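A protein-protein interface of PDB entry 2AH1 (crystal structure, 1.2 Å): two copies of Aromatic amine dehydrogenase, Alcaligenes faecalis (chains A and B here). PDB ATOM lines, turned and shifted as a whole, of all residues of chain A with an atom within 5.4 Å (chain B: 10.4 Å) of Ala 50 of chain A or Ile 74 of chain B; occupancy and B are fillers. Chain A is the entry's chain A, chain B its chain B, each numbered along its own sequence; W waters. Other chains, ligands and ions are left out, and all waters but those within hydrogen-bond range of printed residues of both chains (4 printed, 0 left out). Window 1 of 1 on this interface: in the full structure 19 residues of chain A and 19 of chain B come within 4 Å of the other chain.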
ATOM      1  N   LEU A  28     -27.558  -0.606 -11.589  1.00  0.00           N
ATOM      2  CA  LEU A  28     -26.562  -1.549 -11.099  1.00  0.00           C
ATOM      3  C   LEU A  28     -26.660  -2.930 -11.746  1.00  0.00           C
ATOM      4  O   LEU A  28     -25.716  -3.700 -11.651  1.00  0.00           O
ATOM      5  CB  LEU A  28     -26.652  -1.614  -9.583  1.00  0.00           C
ATOM      6  CG  LEU A  28     -25.665  -2.463  -8.799  1.00  0.00           C
ATOM      7  CD1 LEU A  28     -24.227  -2.040  -9.052  1.00  0.00           C
ATOM      8  CD2 LEU A  28     -25.977  -2.300  -7.322  1.00  0.00           C
ATOM      9  N   THR A  29     -27.790  -3.232 -12.390  1.00  0.00           N
ATOM     10  CA  THR A  29     -27.899  -4.467 -13.143  1.00  0.00           C
ATOM     11  C   THR A  29     -27.119  -4.451 -14.488  1.00  0.00           C
ATOM     12  O   THR A  29     -27.060  -5.472 -15.152  1.00  0.00           O
ATOM     13  CB  THR A  29     -29.338  -4.886 -13.444  1.00  0.00           C
ATOM     14  OG1 THR A  29     -29.966  -3.953 -14.338  1.00  0.00           O
ATOM     15  CG2 THR A  29     -30.181  -5.054 -12.224  1.00  0.00           C
ATOM     16  N   GLU A  30     -26.555  -3.295 -14.869  1.00  0.00           N
ATOM     17  CA  GLU A  30     -25.756  -3.165 -16.083  1.00  0.00           C
ATOM     18  C   GLU A  30     -24.366  -2.647 -15.801  1.00  0.00           C
ATOM     19  O   GLU A  30     -23.787  -1.874 -16.578  1.00  0.00           O
ATOM     20  CB  GLU A  30     -26.469  -2.331 -17.148  1.00  0.00           C
ATOM     21  CG  GLU A  30     -26.053  -2.721 -18.567  1.00  0.00           C
ATOM     22  CD  GLU A  30     -26.554  -1.759 -19.617  1.00  0.00           C
ATOM     23  OE1 GLU A  30     -27.689  -1.956 -20.137  1.00  0.00           O
ATOM     24  OE2 GLU A  30     -25.808  -0.815 -19.916  1.00  0.00           O
ATOM     25  N   SER A  31     -23.789  -3.109 -14.700  1.00  0.00           N
ATOM     26  CA  SER A  31     -22.395  -2.848 -14.411  1.00  0.00           C
ATOM     27  C   SER A  31     -21.520  -3.434 -15.542  1.00  0.00           C
ATOM     28  O   SER A  31     -21.940  -4.351 -16.261  1.00  0.00           O
ATOM     29  CB  SER A  31     -21.997  -3.449 -13.061  1.00  0.00           C
ATOM     30  OG  SER A  31     -21.960  -4.877 -13.093  1.00  0.00           O
ATOM     31  N   PRO A  48     -19.368  -6.871 -20.154  1.00  0.00           N
ATOM     32  CA  PRO A  48     -20.602  -6.687 -19.350  1.00  0.00           C
ATOM     33  C   PRO A  48     -20.556  -7.584 -18.134  1.00  0.00           C
ATOM     34  O   PRO A  48     -20.125  -8.742 -18.215  1.00  0.00           O
ATOM     35  CB  PRO A  48     -21.703  -7.141 -20.328  1.00  0.00           C
ATOM     36  CG  PRO A  48     -20.999  -8.184 -21.185  1.00  0.00           C
ATOM     37  CD  PRO A  48     -19.624  -7.582 -21.423  1.00  0.00           C
ATOM     38  N   THR A  49     -21.019  -7.053 -16.990  1.00  0.00           N
ATOM     39  CA  THR A  49     -20.944  -7.809 -15.741  1.00  0.00           C
ATOM     40  C   THR A  49     -22.243  -7.773 -14.906  1.00  0.00           C
ATOM     41  O   THR A  49     -22.206  -7.941 -13.696  1.00  0.00           O
ATOM     42  CB  THR A  49     -19.754  -7.399 -14.871  1.00  0.00           C
ATOM     43  OG1 THR A  49     -19.826  -6.003 -14.550  1.00  0.00           O
ATOM     44  CG2 THR A  49     -18.415  -7.604 -15.559  1.00  0.00           C
ATOM     45  N   ALA A  50     -23.385  -7.576 -15.555  1.00  0.00           N
ATOM     46  CA  ALA A  50     -24.683  -7.766 -14.932  1.00  0.00           C
ATOM     47  C   ALA A  50     -24.785  -7.014 -13.631  1.00  0.00           C
ATOM     48  O   ALA A  50     -24.395  -5.854 -13.568  1.00  0.00           O
ATOM     49  CB  ALA A  50     -25.019  -9.253 -14.826  1.00  0.00           C
ATOM     50  N   PHE A  51     -25.341  -7.634 -12.587  1.00  0.00           N
ATOM     51  CA  PHE A  51     -25.574  -6.944 -11.328  1.00  0.00           C
ATOM     52  C   PHE A  51     -24.327  -6.855 -10.467  1.00  0.00           C
ATOM     53  O   PHE A  51     -23.813  -7.864 -10.033  1.00  0.00           O
ATOM     54  CB  PHE A  51     -26.703  -7.600 -10.527  1.00  0.00           C
ATOM     55  CG  PHE A  51     -27.001  -6.902  -9.249  1.00  0.00           C
ATOM     56  CD1 PHE A  51     -27.721  -5.736  -9.253  1.00  0.00           C
ATOM     57  CD2 PHE A  51     -26.549  -7.403  -8.022  1.00  0.00           C
ATOM     58  CE1 PHE A  51     -28.002  -5.085  -8.034  1.00  0.00           C
ATOM     59  CE2 PHE A  51     -26.840  -6.747  -6.830  1.00  0.00           C
ATOM     60  CZ  PHE A  51     -27.552  -5.612  -6.877  1.00  0.00           C
ATOM     61  N   ASN A  52     -23.845  -5.640 -10.228  1.00  0.00           N
ATOM     62  CA  ASN A  52     -22.758  -5.416  -9.293  1.00  0.00           C
ATOM     63  C   ASN A  52     -21.577  -6.349  -9.550  1.00  0.00           C
ATOM     64  O   ASN A  52     -21.155  -7.100  -8.675  1.00  0.00           O
ATOM     65  CB  ASN A  52     -23.252  -5.554  -7.841  1.00  0.00           C
ATOM     66  CG  ASN A  52     -22.171  -5.330  -6.811  1.00  0.00           C
ATOM     67  OD1 ASN A  52     -21.322  -4.405  -6.918  1.00  0.00           O
ATOM     68  ND2 ASN A  52     -22.193  -6.132  -5.804  1.00  0.00           N
ATOM     69  N   GLY A  53     -21.024  -6.304 -10.758  1.00  0.00           N
ATOM     70  CA  GLY A  53     -19.897  -7.165 -11.055  1.00  0.00           C
ATOM     71  C   GLY A  53     -18.638  -6.779 -10.324  1.00  0.00           C
ATOM     72  O   GLY A  53     -18.446  -5.628  -9.955  1.00  0.00           O
ATOM     73  N   THR A  68     -20.344 -12.208 -10.730  1.00  0.00           N
ATOM     74  CA  THR A  68     -21.603 -11.492 -10.815  1.00  0.00           C
ATOM     75  C   THR A  68     -22.757 -12.360 -10.341  1.00  0.00           C
ATOM     76  O   THR A  68     -22.585 -13.515  -9.999  1.00  0.00           O
ATOM     77  CB  THR A  68     -21.808 -10.902 -12.219  1.00  0.00           C
ATOM     78  OG1 THR A  68     -22.941 -10.014 -12.196  1.00  0.00           O
ATOM     79  CG2 THR A  68     -22.088 -11.961 -13.276  1.00  0.00           C
ATOM     80  N   THR A  69     -23.924 -11.740 -10.355  1.00  0.00           N
ATOM     81  CA  THR A  69     -25.188 -12.405 -10.039  1.00  0.00           C
ATOM     82  C   THR A  69     -26.181 -12.198 -11.166  1.00  0.00           C
ATOM     83  O   THR A  69     -26.382 -11.080 -11.608  1.00  0.00           O
ATOM     84  CB  THR A  69     -25.797 -11.816  -8.742  1.00  0.00           C
ATOM     85  OG1 THR A  69     -24.932 -12.107  -7.635  1.00  0.00           O
ATOM     86  CG2 THR A  69     -27.188 -12.371  -8.437  1.00  0.00           C
ATOM     87  N   TYR A  70     -26.820 -13.287 -11.573  1.00  0.00           N
ATOM     88  CA  TYR A  70     -27.948 -13.292 -12.482  1.00  0.00           C
ATOM     89  C   TYR A  70     -29.191 -13.796 -11.766  1.00  0.00           C
ATOM     90  O   TYR A  70     -29.072 -14.549 -10.823  1.00  0.00           O
ATOM     91  CB  TYR A  70     -27.668 -14.232 -13.654  1.00  0.00           C
ATOM     92  CG  TYR A  70     -26.503 -13.874 -14.524  1.00  0.00           C
ATOM     93  CD1 TYR A  70     -25.265 -14.465 -14.325  1.00  0.00           C
ATOM     94  CD2 TYR A  70     -26.637 -12.958 -15.556  1.00  0.00           C
ATOM     95  CE1 TYR A  70     -24.191 -14.149 -15.136  1.00  0.00           C
ATOM     96  CE2 TYR A  70     -25.548 -12.635 -16.383  1.00  0.00           C
ATOM     97  CZ  TYR A  70     -24.340 -13.234 -16.159  1.00  0.00           C
ATOM     98  OH  TYR A  70     -23.260 -12.951 -16.955  1.00  0.00           O
ATOM     99  N   ILE A  74     -34.185 -11.376 -13.845  1.00  0.00           N
ATOM    100  CA  ILE A  74     -33.475 -10.194 -13.295  1.00  0.00           C
ATOM    101  C   ILE A  74     -33.940  -9.856 -11.875  1.00  0.00           C
ATOM    102  O   ILE A  74     -33.184  -9.998 -10.914  1.00  0.00           O
ATOM    103  CB  ILE A  74     -33.536  -8.979 -14.233  1.00  0.00           C
ATOM    104  CG1 ILE A  74     -33.106  -9.332 -15.661  1.00  0.00           C
ATOM    105  CG2 ILE A  74     -32.593  -7.882 -13.698  1.00  0.00           C
ATOM    106  CD1 ILE A  74     -33.480  -8.323 -16.650  1.00  0.00           C
ATOM    107  N   HIS B  27     -28.262   2.583 -20.691  1.00  0.00           N
ATOM    108  CA  HIS B  27     -28.243   1.283 -20.001  1.00  0.00           C
ATOM    109  C   HIS B  27     -29.543   0.558 -20.297  1.00  0.00           C
ATOM    110  O   HIS B  27     -30.325   0.274 -19.373  1.00  0.00           O
ATOM    111  CB  HIS B  27     -27.979   1.444 -18.494  1.00  0.00           C
ATOM    112  CG  HIS B  27     -26.682   2.118 -18.259  1.00  0.00           C
ATOM    113  ND1 HIS B  27     -25.482   1.498 -18.522  1.00  0.00           N
ATOM    114  CD2 HIS B  27     -26.380   3.373 -17.847  1.00  0.00           C
ATOM    115  CE1 HIS B  27     -24.498   2.335 -18.271  1.00  0.00           C
ATOM    116  NE2 HIS B  27     -25.013   3.488 -17.872  1.00  0.00           N
ATOM    117  N   LEU B  28     -29.746   0.248 -21.585  1.00  0.00           N
ATOM    118  CA  LEU B  28     -31.039  -0.119 -22.098  1.00  0.00           C
ATOM    119  C   LEU B  28     -31.548  -1.456 -21.556  1.00  0.00           C
ATOM    120  O   LEU B  28     -32.720  -1.751 -21.696  1.00  0.00           O
ATOM    121  CB  LEU B  28     -30.956  -0.140 -23.620  1.00  0.00           C
ATOM    122  CG  LEU B  28     -32.192  -0.409 -24.479  1.00  0.00           C
ATOM    123  CD1 LEU B  28     -33.295   0.587 -24.142  1.00  0.00           C
ATOM    124  CD2 LEU B  28     -31.847  -0.333 -25.959  1.00  0.00           C
ATOM    125  N   THR B  29     -30.676  -2.263 -20.957  1.00  0.00           N
ATOM    126  CA  THR B  29     -31.101  -3.478 -20.282  1.00  0.00           C
ATOM    127  C   THR B  29     -31.819  -3.214 -18.957  1.00  0.00           C
ATOM    128  O   THR B  29     -32.322  -4.160 -18.352  1.00  0.00           O
ATOM    129  CB  THR B  29     -29.978  -4.488 -20.029  1.00  0.00           C
ATOM    130  OG1 THR B  29     -29.031  -3.968 -19.085  1.00  0.00           O
ATOM    131  CG2 THR B  29     -29.258  -4.914 -21.333  1.00  0.00           C
ATOM    132  N   GLU B  30     -31.853  -1.955 -18.502  1.00  0.00           N
ATOM    133  CA  GLU B  30     -32.523  -1.606 -17.249  1.00  0.00           C
ATOM    134  C   GLU B  30     -33.572  -0.519 -17.460  1.00  0.00           C
ATOM    135  O   GLU B  30     -33.743   0.370 -16.622  1.00  0.00           O
ATOM    136  CB  GLU B  30     -31.532  -1.223 -16.121  1.00  0.00           C
ATOM    137  CG  GLU B  30     -32.076  -1.505 -14.748  1.00  0.00           C
ATOM    138  CD  GLU B  30     -31.260  -0.926 -13.638  1.00  0.00           C
ATOM    139  OE1 GLU B  30     -30.351  -1.608 -13.142  1.00  0.00           O
ATOM    140  OE2 GLU B  30     -31.562   0.220 -13.235  1.00  0.00           O
ATOM    141  N   SER B  31     -34.283  -0.611 -18.564  1.00  0.00           N
ATOM    142  CA  SER B  31     -35.423   0.227 -18.828  1.00  0.00           C
ATOM    143  C   SER B  31     -36.472   0.003 -17.733  1.00  0.00           C
ATOM    144  O   SER B  31     -36.499  -1.037 -17.097  1.00  0.00           O
ATOM    145  CB  SER B  31     -36.001  -0.052 -20.214  1.00  0.00           C
ATOM    146  OG  SER B  31     -36.653  -1.314 -20.292  1.00  0.00           O
ATOM    147  N   ALA B  50     -36.550  -4.497 -18.013  1.00  0.00           N
ATOM    148  CA  ALA B  50     -35.452  -5.203 -18.680  1.00  0.00           C
ATOM    149  C   ALA B  50     -35.013  -4.482 -19.952  1.00  0.00           C
ATOM    150  O   ALA B  50     -34.863  -3.247 -19.917  1.00  0.00           O
ATOM    151  CB  ALA B  50     -35.806  -6.667 -18.899  1.00  0.00           C
ATOM    152  N   PHE B  51     -34.760  -5.203 -21.042  1.00  0.00           N
ATOM    153  CA  PHE B  51     -34.217  -4.578 -22.239  1.00  0.00           C
ATOM    154  C   PHE B  51     -35.300  -3.912 -23.070  1.00  0.00           C
ATOM    155  O   PHE B  51     -36.192  -4.582 -23.568  1.00  0.00           O
ATOM    156  CB  PHE B  51     -33.481  -5.601 -23.124  1.00  0.00           C
ATOM    157  CG  PHE B  51     -32.910  -5.023 -24.374  1.00  0.00           C
ATOM    158  CD1 PHE B  51     -31.745  -4.293 -24.320  1.00  0.00           C
ATOM    159  CD2 PHE B  51     -33.528  -5.206 -25.603  1.00  0.00           C
ATOM    160  CE1 PHE B  51     -31.225  -3.767 -25.456  1.00  0.00           C
ATOM    161  CE2 PHE B  51     -32.983  -4.666 -26.741  1.00  0.00           C
ATOM    162  CZ  PHE B  51     -31.836  -3.948 -26.666  1.00  0.00           C
ATOM    163  N   ASN B  52     -35.227  -2.591 -23.207  1.00  0.00           N
ATOM    164  CA  ASN B  52     -36.131  -1.863 -24.109  1.00  0.00           C
ATOM    165  C   ASN B  52     -37.584  -2.207 -23.918  1.00  0.00           C
ATOM    166  O   ASN B  52     -38.261  -2.632 -24.857  1.00  0.00           O
ATOM    167  CB  ASN B  52     -35.726  -2.116 -25.565  1.00  0.00           C
ATOM    168  CG  ASN B  52     -36.560  -1.359 -26.577  1.00  0.00           C
ATOM    169  OD1 ASN B  52     -36.911  -0.176 -26.412  1.00  0.00           O
ATOM    170  ND2 ASN B  52     -36.867  -2.029 -27.644  1.00  0.00           N
ATOM    171  N   THR B  68     -41.196  -7.014 -23.114  1.00  0.00           N
ATOM    172  CA  THR B  68     -39.767  -6.918 -22.996  1.00  0.00           C
ATOM    173  C   THR B  68     -39.097  -8.177 -23.510  1.00  0.00           C
ATOM    174  O   THR B  68     -39.758  -9.119 -23.918  1.00  0.00           O
ATOM    175  CB  THR B  68     -39.379  -6.573 -21.548  1.00  0.00           C
ATOM    176  OG1 THR B  68     -37.970  -6.278 -21.521  1.00  0.00           O
ATOM    177  CG2 THR B  68     -39.646  -7.698 -20.567  1.00  0.00           C
ATOM    178  N   THR B  69     -37.764  -8.133 -23.483  1.00  0.00           N
ATOM    179  CA  THR B  69     -36.891  -9.246 -23.886  1.00  0.00           C
ATOM    180  C   THR B  69     -35.929  -9.562 -22.772  1.00  0.00           C
ATOM    181  O   THR B  69     -35.286  -8.639 -22.226  1.00  0.00           O
ATOM    182  CB  THR B  69     -36.069  -8.856 -25.134  1.00  0.00           C
ATOM    183  OG1 THR B  69     -36.948  -8.701 -26.249  1.00  0.00           O
ATOM    184  CG2 THR B  69     -35.012  -9.921 -25.493  1.00  0.00           C
ATOM    185  N   TYR B  70     -35.846 -10.837 -22.434  1.00  0.00           N
ATOM    186  CA  TYR B  70     -34.838 -11.373 -21.552  1.00  0.00           C
ATOM    187  C   TYR B  70     -33.937 -12.338 -22.324  1.00  0.00           C
ATOM    188  O   TYR B  70     -34.337 -12.904 -23.334  1.00  0.00           O
ATOM    189  CB  TYR B  70     -35.484 -12.184 -20.433  1.00  0.00           C
ATOM    190  CG  TYR B  70     -36.423 -11.427 -19.527  1.00  0.00           C
ATOM    191  CD1 TYR B  70     -37.800 -11.408 -19.752  1.00  0.00           C
ATOM    192  CD2 TYR B  70     -35.932 -10.731 -18.449  1.00  0.00           C
ATOM    193  CE1 TYR B  70     -38.656 -10.721 -18.923  1.00  0.00           C
ATOM    194  CE2 TYR B  70     -36.793 -10.037 -17.592  1.00  0.00           C
ATOM    195  CZ  TYR B  70     -38.143 -10.036 -17.846  1.00  0.00           C
ATOM    196  OH  TYR B  70     -38.986  -9.348 -17.005  1.00  0.00           O
ATOM    197  N   HIS B  71     -32.716 -12.532 -21.815  1.00  0.00           N
ATOM    198  CA  HIS B  71     -31.900 -13.683 -22.202  1.00  0.00           C
ATOM    199  C   HIS B  71     -31.387 -14.342 -20.933  1.00  0.00           C
ATOM    200  O   HIS B  71     -31.183 -13.682 -19.915  1.00  0.00           O
ATOM    201  CB  HIS B  71     -30.709 -13.339 -23.129  1.00  0.00           C
ATOM    202  CG  HIS B  71     -31.088 -12.710 -24.421  1.00  0.00           C
ATOM    203  ND1 HIS B  71     -31.113 -13.392 -25.624  1.00  0.00           N
ATOM    204  CD2 HIS B  71     -31.443 -11.443 -24.699  1.00  0.00           C
ATOM    205  CE1 HIS B  71     -31.475 -12.556 -26.582  1.00  0.00           C
ATOM    206  NE2 HIS B  71     -31.677 -11.368 -26.045  1.00  0.00           N
ATOM    207  N   GLU B  72     -31.132 -15.643 -21.002  1.00  0.00           N
ATOM    208  CA  GLU B  72     -30.726 -16.355 -19.812  1.00  0.00           C
ATOM    209  C   GLU B  72     -29.547 -15.730 -19.074  1.00  0.00           C
ATOM    210  O   GLU B  72     -29.469 -15.767 -17.845  1.00  0.00           O
ATOM    211  CB  GLU B  72     -30.381 -17.802 -20.135  1.00  0.00           C
ATOM    212  CG  GLU B  72     -31.475 -18.688 -20.684  1.00  0.00           C
ATOM    213  CD  GLU B  72     -30.941 -20.062 -21.145  1.00  0.00           C
ATOM    214  OE1 GLU B  72     -30.015 -20.159 -22.038  1.00  0.00           O
ATOM    215  OE2 GLU B  72     -31.460 -21.071 -20.611  1.00  0.00           O
ATOM    216  N   ARG B  73     -28.603 -15.169 -19.830  1.00  0.00           N
ATOM    217  CA  ARG B  73     -27.466 -14.490 -19.247  1.00  0.00           C
ATOM    218  C   ARG B  73     -27.297 -13.080 -19.837  1.00  0.00           C
ATOM    219  O   ARG B  73     -26.182 -12.578 -19.935  1.00  0.00           O
ATOM    220  CB  ARG B  73     -26.207 -15.350 -19.418  1.00  0.00           C
ATOM    221  CG  ARG B  73     -26.223 -16.623 -18.601  1.00  0.00           C
ATOM    222  CD  ARG B  73     -25.942 -16.369 -17.147  1.00  0.00           C
ATOM    223  NE  ARG B  73     -25.782 -17.606 -16.403  1.00  0.00           N
ATOM    224  CZ  ARG B  73     -26.765 -18.258 -15.853  1.00  0.00           C
ATOM    225  NH1 ARG B  73     -28.000 -17.792 -15.943  1.00  0.00           N
ATOM    226  NH2 ARG B  73     -26.520 -19.386 -15.178  1.00  0.00           N
ATOM    227  N   ILE B  74     -28.428 -12.470 -20.197  1.00  0.00           N
ATOM    228  CA  ILE B  74     -28.553 -11.087 -20.635  1.00  0.00           C
ATOM    229  C   ILE B  74     -27.970 -10.858 -22.037  1.00  0.00           C
ATOM    230  O   ILE B  74     -28.702 -10.583 -22.982  1.00  0.00           O
ATOM    231  CB  ILE B  74     -27.985 -10.059 -19.600  1.00  0.00           C
ATOM    232  CG1 ILE B  74     -28.538 -10.303 -18.182  1.00  0.00           C
ATOM    233  CG2 ILE B  74     -28.293  -8.658 -20.074  1.00  0.00           C
ATOM    234  CD1 ILE B  74     -27.806  -9.554 -17.139  1.00  0.00           C
ATOM    235  N   THR B  75     -26.653 -10.944 -22.115  1.00  0.00           N
ATOM    236  CA  THR B  75     -25.904 -10.780 -23.354  1.00  0.00           C
ATOM    237  C   THR B  75     -25.555 -12.098 -24.040  1.00  0.00           C
ATOM    238  O   THR B  75     -24.927 -12.112 -25.099  1.00  0.00           O
ATOM    239  CB  THR B  75     -24.620 -10.008 -23.081  1.00  0.00           C
ATOM    240  OG1 THR B  75     -23.974 -10.518 -21.905  1.00  0.00           O
ATOM    241  CG2 THR B  75     -24.959  -8.548 -22.795  1.00  0.00           C
ATOM    242  N   ARG B  76     -25.974 -13.215 -23.460  1.00  0.00           N
ATOM    243  CA  ARG B  76     -25.881 -14.514 -24.082  1.00  0.00           C
ATOM    244  C   ARG B  76     -27.000 -15.383 -23.538  1.00  0.00           C
ATOM    245  O   ARG B  76     -27.678 -15.010 -22.582  1.00  0.00           O
ATOM    246  CB  ARG B  76     -24.506 -15.160 -23.846  1.00  0.00           C
ATOM    247  CG  ARG B  76     -24.175 -15.402 -22.390  1.00  0.00           C
ATOM    248  CD  ARG B  76     -22.736 -15.902 -22.164  1.00  0.00           C
ATOM    249  NE  ARG B  76     -22.495 -15.944 -20.722  1.00  0.00           N
ATOM    250  CZ  ARG B  76     -22.754 -16.950 -19.911  1.00  0.00           C
ATOM    251  NH1 ARG B  76     -23.264 -18.062 -20.375  1.00  0.00           N
ATOM    252  NH2 ARG B  76     -22.521 -16.840 -18.600  1.00  0.00           N
ATOM    253  N   GLY B  77     -27.187 -16.537 -24.159  1.00  0.00           N
ATOM    254  CA  GLY B  77     -28.197 -17.486 -23.721  1.00  0.00           C
ATOM    255  C   GLY B  77     -29.530 -17.282 -24.413  1.00  0.00           C
ATOM    256  O   GLY B  77     -29.715 -16.363 -25.211  1.00  0.00           O
ATOM    257  N   LYS B  78     -30.456 -18.169 -24.103  1.00  0.00           N
ATOM    258  CA  LYS B  78     -31.732 -18.208 -24.785  1.00  0.00           C
ATOM    259  C   LYS B  78     -32.563 -16.955 -24.562  1.00  0.00           C
ATOM    260  O   LYS B  78     -32.662 -16.447 -23.451  1.00  0.00           O
ATOM    261  CB  LYS B  78     -32.537 -19.419 -24.335  1.00  0.00           C
ATOM    262  CG  LYS B  78     -33.801 -19.646 -25.191  1.00  0.00           C
ATOM    263  CD  LYS B  78     -34.614 -20.828 -24.690  1.00  0.00           C
ATOM    264  CE  LYS B  78     -35.958 -20.974 -25.409  1.00  0.00           C
ATOM    265  NZ  LYS B  78     -35.819 -21.006 -26.888  1.00  0.00           N
ATOM    266  N   ARG B  79     -33.153 -16.475 -25.657  1.00  0.00           N
ATOM    267  CA  ARG B  79     -34.066 -15.320 -25.649  1.00  0.00           C
ATOM    268  C   ARG B  79     -35.483 -15.672 -25.223  1.00  0.00           C
ATOM    269  O   ARG B  79     -36.020 -16.676 -25.665  1.00  0.00           O
ATOM    270  CB  ARG B  79     -34.117 -14.720 -27.061  1.00  0.00           C
ATOM    271  CG  ARG B  79     -34.996 -13.491 -27.230  1.00  0.00           C
ATOM    272  CD  ARG B  79     -34.657 -12.750 -28.491  1.00  0.00           C
ATOM    273  NE  ARG B  79     -35.675 -11.785 -28.867  1.00  0.00           N
ATOM    274  CZ  ARG B  79     -35.585 -10.988 -29.927  1.00  0.00           C
ATOM    275  NH1 ARG B  79     -34.509 -11.027 -30.685  1.00  0.00           N
ATOM    276  NH2 ARG B  79     -36.563 -10.156 -30.218  1.00  0.00           N
ATOM    277  N   SER B  80     -36.071 -14.835 -24.357  1.00  0.00           N
ATOM    278  CA  SER B  80     -37.491 -14.910 -24.064  1.00  0.00           C
ATOM    279  C   SER B  80     -38.108 -13.528 -24.262  1.00  0.00           C
ATOM    280  O   SER B  80     -37.828 -12.617 -23.466  1.00  0.00           O
ATOM    281  CB  SER B  80     -37.725 -15.349 -22.607  1.00  0.00           C
ATOM    282  OG  SER B  80     -37.206 -16.631 -22.369  1.00  0.00           O
ATOM    283  N   ASP B  81     -38.930 -13.375 -25.294  1.00  0.00           N
ATOM    284  CA  ASP B  81     -39.772 -12.201 -25.452  1.00  0.00           C
ATOM    285  C   ASP B  81     -41.096 -12.458 -24.733  1.00  0.00           C
ATOM    286  O   ASP B  81     -41.667 -13.530 -24.865  1.00  0.00           O
ATOM    287  CB  ASP B  81     -40.037 -11.910 -26.923  1.00  0.00           C
ATOM    288  CG  ASP B  81     -38.871 -11.343 -27.626  1.00  0.00           C
ATOM    289  OD1 ASP B  81     -37.800 -11.125 -27.007  1.00  0.00           O
ATOM    290  OD2 ASP B  81     -38.970 -11.111 -28.847  1.00  0.00           O
ATOM    291  N   GLN B 105     -38.145  -4.417 -31.141  1.00  0.00           N
ATOM    292  CA  GLN B 105     -37.195  -3.719 -30.308  1.00  0.00           C
ATOM    293  C   GLN B 105     -36.952  -2.368 -31.000  1.00  0.00           C
ATOM    294  O   GLN B 105     -36.410  -2.263 -32.112  1.00  0.00           O
ATOM    295  CB  GLN B 105     -35.926  -4.533 -30.170  1.00  0.00           C
ATOM    296  CG  GLN B 105     -36.184  -5.852 -29.445  1.00  0.00           C
ATOM    297  CD  GLN B 105     -34.970  -6.732 -29.301  1.00  0.00           C
ATOM    298  OE1 GLN B 105     -34.956  -7.675 -28.441  1.00  0.00           O
ATOM    299  NE2 GLN B 105     -33.972  -6.468 -30.091  1.00  0.00           N
HETATM  300  O   HOH W   1     -27.716  -5.953 -17.762  1.00  0.00           O
HETATM  301  O   HOH W   2     -21.618 -13.262 -19.878  1.00  0.00           O
HETATM  302  O   HOH W   3     -31.994  -5.074 -15.769  1.00  0.00           O
HETATM  303  O   HOH W   4     -23.768 -12.078 -19.230  1.00  0.00           O
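Of chain B, only Ile 74 comes within 4 Å of Ala 50 of chain A.
Ile 74 of chain B touches just these residues of chain A: Ala 50 and Tyr 70.
Of chain B, only Glu 30 (2.7 Å) comes within 4 Å of Thr 29 of chain A.
No residue of chain B comes within 4 Å of Ser 31 of chain A.
No residue of chain B comes within 4 Å of Thr 49 of chain A.
Printed residues of chain A within 4 Å of Leu 28 of chain B: Glu 30 (3.3 Å).
Printed residues of chain A within 4 Å of Ala 50 of chain B: Ile 74 (3.6 Å).
Of the printed residues of chain B, Glu 30 of chain A touches His 27 (2.7 Å), Leu 28 (3.3 Å) and Thr 29 (2.6 Å).
Printed residues of chain B within 4 Å of Ile 74 of chain A: Ala 50 and Tyr 70.
Lys 78 of chain B touches none of the printed residues of chain A.
The nearest residue of chain A that does not touch Ile 74 of chain B is Thr 29 of chain A (4.6 Å).
Water W4 lies within hydrogen-bond range of OH of Tyr 70 of chain A (2.5 Å), O of Arg 73 of chain B (2.6 Å) and OG1 of Thr 75 of chain B (3.1 Å).
Water W3 lies within hydrogen-bond range of OG1 of Thr 29 of chain A (2.7 Å) and O of Thr 29 of chain B (2.8 Å).
Water W1 bridges OG1 of Thr 29 of chain B (2.7 Å) and O of Thr 29 of chain A (2.7 Å).
Of the 23 printed residues of chain B, 9 touch a printed residue of chain A.
Printed residues of chain B that touch a printed residue of chain A: His 27, Leu 28, Thr 29, Glu 30, Ala 50, Tyr 70, Arg 73, Ile 74 and Thr 75.
Hydrophobic or aromatic side chains of chain B within 4 Å of the printed part of chain A: His 27, Ala 50, Tyr 70 and Ile 74.
Among the printed residues, 11 pairs touch across the chains.
Among the printed residues, no Asp or Glu carboxylate lies within 4 Å of a Lys or Arg side-chain nitrogen of the other chain.
O of Tyr 70 of chain B is in hydrogen-bond range of N of Ser 80 of chain B (2.8 Å).
The side-chain hydroxyl (OG) of Ser 31 of chain A sits at hydrogen-bond distance from the backbone carbonyl oxygen (O) of Ala 50 of chain A (2.7 Å).
O of Ala 50 of chain B sits at hydrogen-bond distance from OG of Ser 31 of chain B (2.7 Å).
The side-chain hydroxyl (OG1) of Thr 29 of chain A lies within hydrogen-bond range of the side-chain carboxylate (OE1) of Glu 30 of chain B (2.7 Å).
OE1 of Glu 30 of chain A is in hydrogen-bond range of OG1 of Thr 29 of chain B (2.6 Å).
ND1 of His 27 of chain B sits at hydrogen-bond distance from OE2 of Glu 30 of chain A, at 2.7 Å.
The backbone NH (N) of Leu 28 of chain A sits at hydrogen-bond distance from the side-chain carboxylate (OE1) of Glu 30 of chain B.
The side-chain carboxylate (OE1) of Glu 30 of chain A is in hydrogen-bond range of the backbone NH (N) of Leu 28 of chain B, at 3.3 Å.
Leu 28 of chain A touches Glu 30 of chain B, and with the chains exchanged Glu 30 of chain A touches Leu 28 of chain B.
Tyr 70 of chain A touches Ile 74 of chain B, and with the chains exchanged Ile 74 of chain A touches Tyr 70 of chain B.
11 positions are printed for both chains.
Of the 11 pairs that touch across the chains among the printed residues, 8 have their exchanged pair printed and touching as well.
CG of Pro 48 of chain A touches OG1 of Thr 75 of chain B (3.8 Å).
CB of Ala 50 of chain A touches CD1 of Ile 74 of chain B, at 3.6 Å.
CD of Arg 73 of chain B touches CE1 of Tyr 70 of chain A, 3.5 Å away.
Tyr 70 of chain A touches Ile 74 of chain B (CE2 to CD1, 3.9 Å).
Ile 74 of chain A touches Ala 50 of chain B (CD1 to CB, 3.6 Å).
CE2 of Tyr 70 of chain B touches CD1 of Ile 74 of chain A, at 3.8 Å.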
